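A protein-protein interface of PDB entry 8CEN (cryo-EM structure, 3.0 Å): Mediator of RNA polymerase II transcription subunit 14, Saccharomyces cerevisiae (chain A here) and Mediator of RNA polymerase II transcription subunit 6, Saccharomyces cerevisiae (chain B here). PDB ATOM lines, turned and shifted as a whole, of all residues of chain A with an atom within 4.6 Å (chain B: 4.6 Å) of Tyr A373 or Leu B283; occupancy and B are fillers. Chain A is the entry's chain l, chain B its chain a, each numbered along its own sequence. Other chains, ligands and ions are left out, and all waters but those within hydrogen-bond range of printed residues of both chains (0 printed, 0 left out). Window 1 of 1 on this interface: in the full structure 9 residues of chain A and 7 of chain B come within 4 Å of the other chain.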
ATOM      1  N   ASN A 344      -9.135  18.781 -16.992  1.00  0.00           N
ATOM      2  CA  ASN A 344      -9.631  17.444 -17.324  1.00  0.00           C
ATOM      3  C   ASN A 344      -9.642  17.248 -18.843  1.00  0.00           C
ATOM      4  O   ASN A 344     -10.679  17.287 -19.512  1.00  0.00           O
ATOM      5  CB  ASN A 344     -10.991  17.210 -16.665  1.00  0.00           C
ATOM      6  CG  ASN A 344     -12.039  18.270 -17.024  1.00  0.00           C
ATOM      7  OD1 ASN A 344     -11.803  19.166 -17.836  1.00  0.00           O
ATOM      8  ND2 ASN A 344     -13.210  18.158 -16.411  1.00  0.00           N
ATOM      9  N   PHE A 369     -19.391  28.604 -25.227  1.00  0.00           N
ATOM     10  CA  PHE A 369     -19.027  27.679 -24.159  1.00  0.00           C
ATOM     11  C   PHE A 369     -17.679  28.039 -23.542  1.00  0.00           C
ATOM     12  O   PHE A 369     -17.542  28.058 -22.315  1.00  0.00           O
ATOM     13  CB  PHE A 369     -18.997  26.241 -24.681  1.00  0.00           C
ATOM     14  CG  PHE A 369     -18.098  25.334 -23.885  1.00  0.00           C
ATOM     15  CD1 PHE A 369     -18.460  24.930 -22.608  1.00  0.00           C
ATOM     16  CD2 PHE A 369     -16.889  24.894 -24.405  1.00  0.00           C
ATOM     17  CE1 PHE A 369     -17.637  24.111 -21.866  1.00  0.00           C
ATOM     18  CE2 PHE A 369     -16.061  24.072 -23.665  1.00  0.00           C
ATOM     19  CZ  PHE A 369     -16.436  23.684 -22.393  1.00  0.00           C
ATOM     20  N   LEU A 370     -16.679  28.345 -24.372  1.00  0.00           N
ATOM     21  CA  LEU A 370     -15.344  28.591 -23.841  1.00  0.00           C
ATOM     22  C   LEU A 370     -15.267  29.932 -23.122  1.00  0.00           C
ATOM     23  O   LEU A 370     -14.565  30.055 -22.110  1.00  0.00           O
ATOM     24  CB  LEU A 370     -14.311  28.512 -24.965  1.00  0.00           C
ATOM     25  CG  LEU A 370     -12.858  28.298 -24.540  1.00  0.00           C
ATOM     26  CD1 LEU A 370     -12.761  27.271 -23.420  1.00  0.00           C
ATOM     27  CD2 LEU A 370     -12.035  27.851 -25.731  1.00  0.00           C
ATOM     28  N   HIS A 371     -15.986  30.945 -23.619  1.00  0.00           N
ATOM     29  CA  HIS A 371     -16.039  32.235 -22.941  1.00  0.00           C
ATOM     30  C   HIS A 371     -16.713  32.103 -21.581  1.00  0.00           C
ATOM     31  O   HIS A 371     -16.213  32.620 -20.569  1.00  0.00           O
ATOM     32  CB  HIS A 371     -16.775  33.244 -23.825  1.00  0.00           C
ATOM     33  CG  HIS A 371     -16.748  34.648 -23.305  1.00  0.00           C
ATOM     34  ND1 HIS A 371     -15.908  35.047 -22.288  1.00  0.00           N
ATOM     35  CD2 HIS A 371     -17.481  35.737 -23.636  1.00  0.00           C
ATOM     36  CE1 HIS A 371     -16.107  36.328 -22.033  1.00  0.00           C
ATOM     37  NE2 HIS A 371     -17.057  36.770 -22.837  1.00  0.00           N
ATOM     38  N   LYS A 372     -17.840  31.379 -21.533  1.00  0.00           N
ATOM     39  CA  LYS A 372     -18.516  31.138 -20.263  1.00  0.00           C
ATOM     40  C   LYS A 372     -17.638  30.327 -19.315  1.00  0.00           C
ATOM     41  O   LYS A 372     -17.638  30.568 -18.104  1.00  0.00           O
ATOM     42  CB  LYS A 372     -19.849  30.432 -20.511  1.00  0.00           C
ATOM     43  CG  LYS A 372     -20.758  30.354 -19.298  1.00  0.00           C
ATOM     44  CD  LYS A 372     -22.097  29.736 -19.667  1.00  0.00           C
ATOM     45  CE  LYS A 372     -23.038  29.692 -18.472  1.00  0.00           C
ATOM     46  NZ  LYS A 372     -24.330  29.027 -18.800  1.00  0.00           N
ATOM     47  N   TYR A 373     -16.846  29.398 -19.856  1.00  0.00           N
ATOM     48  CA  TYR A 373     -16.000  28.556 -19.016  1.00  0.00           C
ATOM     49  C   TYR A 373     -14.845  29.347 -18.408  1.00  0.00           C
ATOM     50  O   TYR A 373     -14.563  29.219 -17.209  1.00  0.00           O
ATOM     51  CB  TYR A 373     -15.474  27.380 -19.836  1.00  0.00           C
ATOM     52  CG  TYR A 373     -14.977  26.221 -19.007  1.00  0.00           C
ATOM     53  CD1 TYR A 373     -15.839  25.199 -18.632  1.00  0.00           C
ATOM     54  CD2 TYR A 373     -13.648  26.140 -18.608  1.00  0.00           C
ATOM     55  CE1 TYR A 373     -15.396  24.132 -17.875  1.00  0.00           C
ATOM     56  CE2 TYR A 373     -13.195  25.073 -17.852  1.00  0.00           C
ATOM     57  CZ  TYR A 373     -14.076  24.074 -17.490  1.00  0.00           C
ATOM     58  OH  TYR A 373     -13.641  23.010 -16.739  1.00  0.00           O
ATOM     59  N   VAL A 374     -14.167  30.173 -19.214  1.00  0.00           N
ATOM     60  CA  VAL A 374     -13.052  30.949 -18.672  1.00  0.00           C
ATOM     61  C   VAL A 374     -13.557  32.027 -17.716  1.00  0.00           C
ATOM     62  O   VAL A 374     -12.888  32.348 -16.723  1.00  0.00           O
ATOM     63  CB  VAL A 374     -12.173  31.538 -19.797  1.00  0.00           C
ATOM     64  CG1 VAL A 374     -11.547  30.421 -20.624  1.00  0.00           C
ATOM     65  CG2 VAL A 374     -12.945  32.503 -20.687  1.00  0.00           C
ATOM     66  N   LEU A 375     -14.755  32.571 -17.951  1.00  0.00           N
ATOM     67  CA  LEU A 375     -15.271  33.548 -16.997  1.00  0.00           C
ATOM     68  C   LEU A 375     -15.779  32.881 -15.724  1.00  0.00           C
ATOM     69  O   LEU A 375     -15.684  33.474 -14.645  1.00  0.00           O
ATOM     70  CB  LEU A 375     -16.339  34.417 -17.661  1.00  0.00           C
ATOM     71  CG  LEU A 375     -15.797  35.761 -18.177  1.00  0.00           C
ATOM     72  CD1 LEU A 375     -14.663  35.602 -19.178  1.00  0.00           C
ATOM     73  CD2 LEU A 375     -16.909  36.574 -18.807  1.00  0.00           C
ATOM     74  N   THR A 376     -16.274  31.640 -15.811  1.00  0.00           N
ATOM     75  CA  THR A 376     -16.570  30.870 -14.605  1.00  0.00           C
ATOM     76  C   THR A 376     -15.297  30.605 -13.808  1.00  0.00           C
ATOM     77  O   THR A 376     -15.297  30.686 -12.571  1.00  0.00           O
ATOM     78  CB  THR A 376     -17.256  29.552 -14.978  1.00  0.00           C
ATOM     79  OG1 THR A 376     -18.482  29.823 -15.667  1.00  0.00           O
ATOM     80  CG2 THR A 376     -17.569  28.725 -13.735  1.00  0.00           C
ATOM     81  N   LEU A 377     -14.199  30.299 -14.510  1.00  0.00           N
ATOM     82  CA  LEU A 377     -12.894  30.163 -13.866  1.00  0.00           C
ATOM     83  C   LEU A 377     -12.492  31.446 -13.147  1.00  0.00           C
ATOM     84  O   LEU A 377     -11.993  31.403 -12.016  1.00  0.00           O
ATOM     85  CB  LEU A 377     -11.835  29.797 -14.906  1.00  0.00           C
ATOM     86  CG  LEU A 377     -11.579  28.335 -15.269  1.00  0.00           C
ATOM     87  CD1 LEU A 377     -10.836  28.270 -16.588  1.00  0.00           C
ATOM     88  CD2 LEU A 377     -10.767  27.652 -14.184  1.00  0.00           C
ATOM     89  N   MET B 279     -11.271  19.970  -9.035  1.00  0.00           N
ATOM     90  CA  MET B 279     -12.300  20.994  -9.088  1.00  0.00           C
ATOM     91  C   MET B 279     -12.920  21.141 -10.482  1.00  0.00           C
ATOM     92  O   MET B 279     -13.934  21.835 -10.637  1.00  0.00           O
ATOM     93  CB  MET B 279     -11.647  22.273  -8.538  1.00  0.00           C
ATOM     94  CG  MET B 279     -12.430  23.542  -8.395  1.00  0.00           C
ATOM     95  SD  MET B 279     -12.550  24.490  -9.903  1.00  0.00           S
ATOM     96  CE  MET B 279     -10.871  25.105 -10.026  1.00  0.00           C
ATOM     97  N   LEU B 280     -12.400  20.403 -11.464  1.00  0.00           N
ATOM     98  CA  LEU B 280     -12.811  20.563 -12.857  1.00  0.00           C
ATOM     99  C   LEU B 280     -14.258  20.119 -13.078  1.00  0.00           C
ATOM    100  O   LEU B 280     -14.962  20.684 -13.926  1.00  0.00           O
ATOM    101  CB  LEU B 280     -11.854  19.779 -13.755  1.00  0.00           C
ATOM    102  CG  LEU B 280     -10.624  20.468 -14.368  1.00  0.00           C
ATOM    103  CD1 LEU B 280     -11.018  21.385 -15.510  1.00  0.00           C
ATOM    104  CD2 LEU B 280      -9.812  21.246 -13.335  1.00  0.00           C
ATOM    105  N   ASP B 281     -14.722  19.111 -12.332  1.00  0.00           N
ATOM    106  CA  ASP B 281     -16.124  18.705 -12.437  1.00  0.00           C
ATOM    107  C   ASP B 281     -17.051  19.778 -11.879  1.00  0.00           C
ATOM    108  O   ASP B 281     -18.160  19.980 -12.391  1.00  0.00           O
ATOM    109  CB  ASP B 281     -16.360  17.374 -11.720  1.00  0.00           C
ATOM    110  CG  ASP B 281     -15.852  17.372 -10.292  1.00  0.00           C
ATOM    111  OD1 ASP B 281     -15.229  18.370  -9.870  1.00  0.00           O
ATOM    112  OD2 ASP B 281     -16.096  16.372  -9.585  1.00  0.00           O
ATOM    113  N   LYS B 282     -16.620  20.462 -10.816  1.00  0.00           N
ATOM    114  CA  LYS B 282     -17.373  21.609 -10.321  1.00  0.00           C
ATOM    115  C   LYS B 282     -17.400  22.733 -11.348  1.00  0.00           C
ATOM    116  O   LYS B 282     -18.422  23.415 -11.503  1.00  0.00           O
ATOM    117  CB  LYS B 282     -16.784  22.079  -8.992  1.00  0.00           C
ATOM    118  CG  LYS B 282     -16.821  20.991  -7.936  1.00  0.00           C
ATOM    119  CD  LYS B 282     -18.254  20.584  -7.645  1.00  0.00           C
ATOM    120  CE  LYS B 282     -18.338  19.680  -6.431  1.00  0.00           C
ATOM    121  NZ  LYS B 282     -17.716  18.356  -6.715  1.00  0.00           N
ATOM    122  N   LEU B 283     -16.294  22.924 -12.079  1.00  0.00           N
ATOM    123  CA  LEU B 283     -16.302  23.878 -13.193  1.00  0.00           C
ATOM    124  C   LEU B 283     -17.315  23.476 -14.251  1.00  0.00           C
ATOM    125  O   LEU B 283     -18.037  24.324 -14.787  1.00  0.00           O
ATOM    126  CB  LEU B 283     -14.922  23.978 -13.833  1.00  0.00           C
ATOM    127  CG  LEU B 283     -13.840  24.748 -13.096  1.00  0.00           C
ATOM    128  CD1 LEU B 283     -12.458  24.340 -13.569  1.00  0.00           C
ATOM    129  CD2 LEU B 283     -14.024  26.256 -13.197  1.00  0.00           C
ATOM    130  N   MET B 284     -17.366  22.183 -14.567  1.00  0.00           N
ATOM    131  CA  MET B 284     -18.287  21.686 -15.581  1.00  0.00           C
ATOM    132  C   MET B 284     -19.738  21.911 -15.173  1.00  0.00           C
ATOM    133  O   MET B 284     -20.549  22.406 -15.965  1.00  0.00           O
ATOM    134  CB  MET B 284     -18.019  20.205 -15.831  1.00  0.00           C
ATOM    135  CG  MET B 284     -18.818  19.627 -16.976  1.00  0.00           C
ATOM    136  SD  MET B 284     -18.356  20.341 -18.560  1.00  0.00           S
ATOM    137  CE  MET B 284     -19.845  20.050 -19.516  1.00  0.00           C
ATOM    138  N   VAL B 285     -20.070  21.586 -13.922  1.00  0.00           N
ATOM    139  CA  VAL B 285     -21.459  21.687 -13.486  1.00  0.00           C
ATOM    140  C   VAL B 285     -21.861  23.148 -13.269  1.00  0.00           C
ATOM    141  O   VAL B 285     -23.041  23.495 -13.412  1.00  0.00           O
ATOM    142  CB  VAL B 285     -21.697  20.820 -12.232  1.00  0.00           C
ATOM    143  CG1 VAL B 285     -21.019  21.401 -10.998  1.00  0.00           C
ATOM    144  CG2 VAL B 285     -23.187  20.609 -11.986  1.00  0.00           C
ATOM    145  N   THR B 286     -20.908  24.034 -12.953  1.00  0.00           N
ATOM    146  CA  THR B 286     -21.261  25.444 -12.828  1.00  0.00           C
ATOM    147  C   THR B 286     -21.386  26.119 -14.187  1.00  0.00           C
ATOM    148  O   THR B 286     -22.295  26.932 -14.395  1.00  0.00           O
ATOM    149  CB  THR B 286     -20.233  26.175 -11.964  1.00  0.00           C
ATOM    150  OG1 THR B 286     -18.912  25.799 -12.366  1.00  0.00           O
ATOM    151  CG2 THR B 286     -20.435  25.831 -10.495  1.00  0.00           C
ATOM    152  N   SER B 287     -20.490  25.803 -15.127  1.00  0.00           N
ATOM    153  CA  SER B 287     -20.548  26.420 -16.444  1.00  0.00           C
ATOM    154  C   SER B 287     -21.674  25.856 -17.298  1.00  0.00           C
ATOM    155  O   SER B 287     -22.133  26.537 -18.221  1.00  0.00           O
ATOM    156  CB  SER B 287     -19.208  26.252 -17.165  1.00  0.00           C
ATOM    157  OG  SER B 287     -19.247  26.840 -18.453  1.00  0.00           O
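Tyr A373 touches just these residues of chain B: Leu B280 (3.3 Å), Leu B283 (3.3 Å) and Ser B287 (3.7 Å).
Of the printed residues of chain A, Leu B283 touches Tyr A373 (3.3 Å) and Leu A377 (3.7 Å).
Of the printed residues of chain B, Lys A372 touches Ser B287.
Of the printed residues of chain B, Leu A377 touches Leu B283 (3.7 Å).
The nearest residue of chain B that does not touch Tyr A373 is Met B284 (4.3 Å).
The nearest printed residue of chain B that does not touch Leu A377 is Met B279 (4.9 Å).
O of Ser B287 sits close to NZ of Lys A372, at 3.4 Å.
Of the 10 printed residues of chain A, 5 touch a printed residue of chain B.
Printed residues of chain A that touch a printed residue of chain B: Asn A344, Lys A372, Tyr A373, Thr A376 and Leu A377.
Hydrophobic or aromatic side chains of chain A within 4 Å of the printed part of chain B: Tyr A373 and Leu A377.
Along chain A the printed residues that touch a printed residue of chain B span positions 344 to 377.
Of the 9 printed residues of chain B, 4 touch a printed residue of chain A.
Hydrophobic or aromatic side chains of chain B that line the printed part of chain A: Leu B280 and Leu B283.
Among the printed residues, no Asp or Glu carboxylate lies within 4 Å of a Lys or Arg side-chain nitrogen of the other chain.
Among the printed residues, merely in contact across the chains: Asn A344 with Leu B280 (3.3 Å), Tyr A373 with Leu B283 (3.3 Å), Tyr A373 with Leu B280 (3.3 Å), Thr A376 with Thr B286 (3.5 Å), Leu A377 with Leu B283 (3.7 Å), Tyr A373 with Ser B287 (3.7 Å) and Thr A376 with Ser B287 (3.9 Å).
The side-chain hydroxyl (OG1) of Thr B286 sits at hydrogen-bond distance from the backbone carbonyl oxygen (O) of Lys B282, at 2.6 Å.
The backbone carbonyl oxygen (O) of Leu B283 lies within hydrogen-bond range of the side-chain hydroxyl (OG1) of Thr B286 (3.0 Å).
O of Lys A372 lies within hydrogen-bond range of OG1 of Thr A376.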
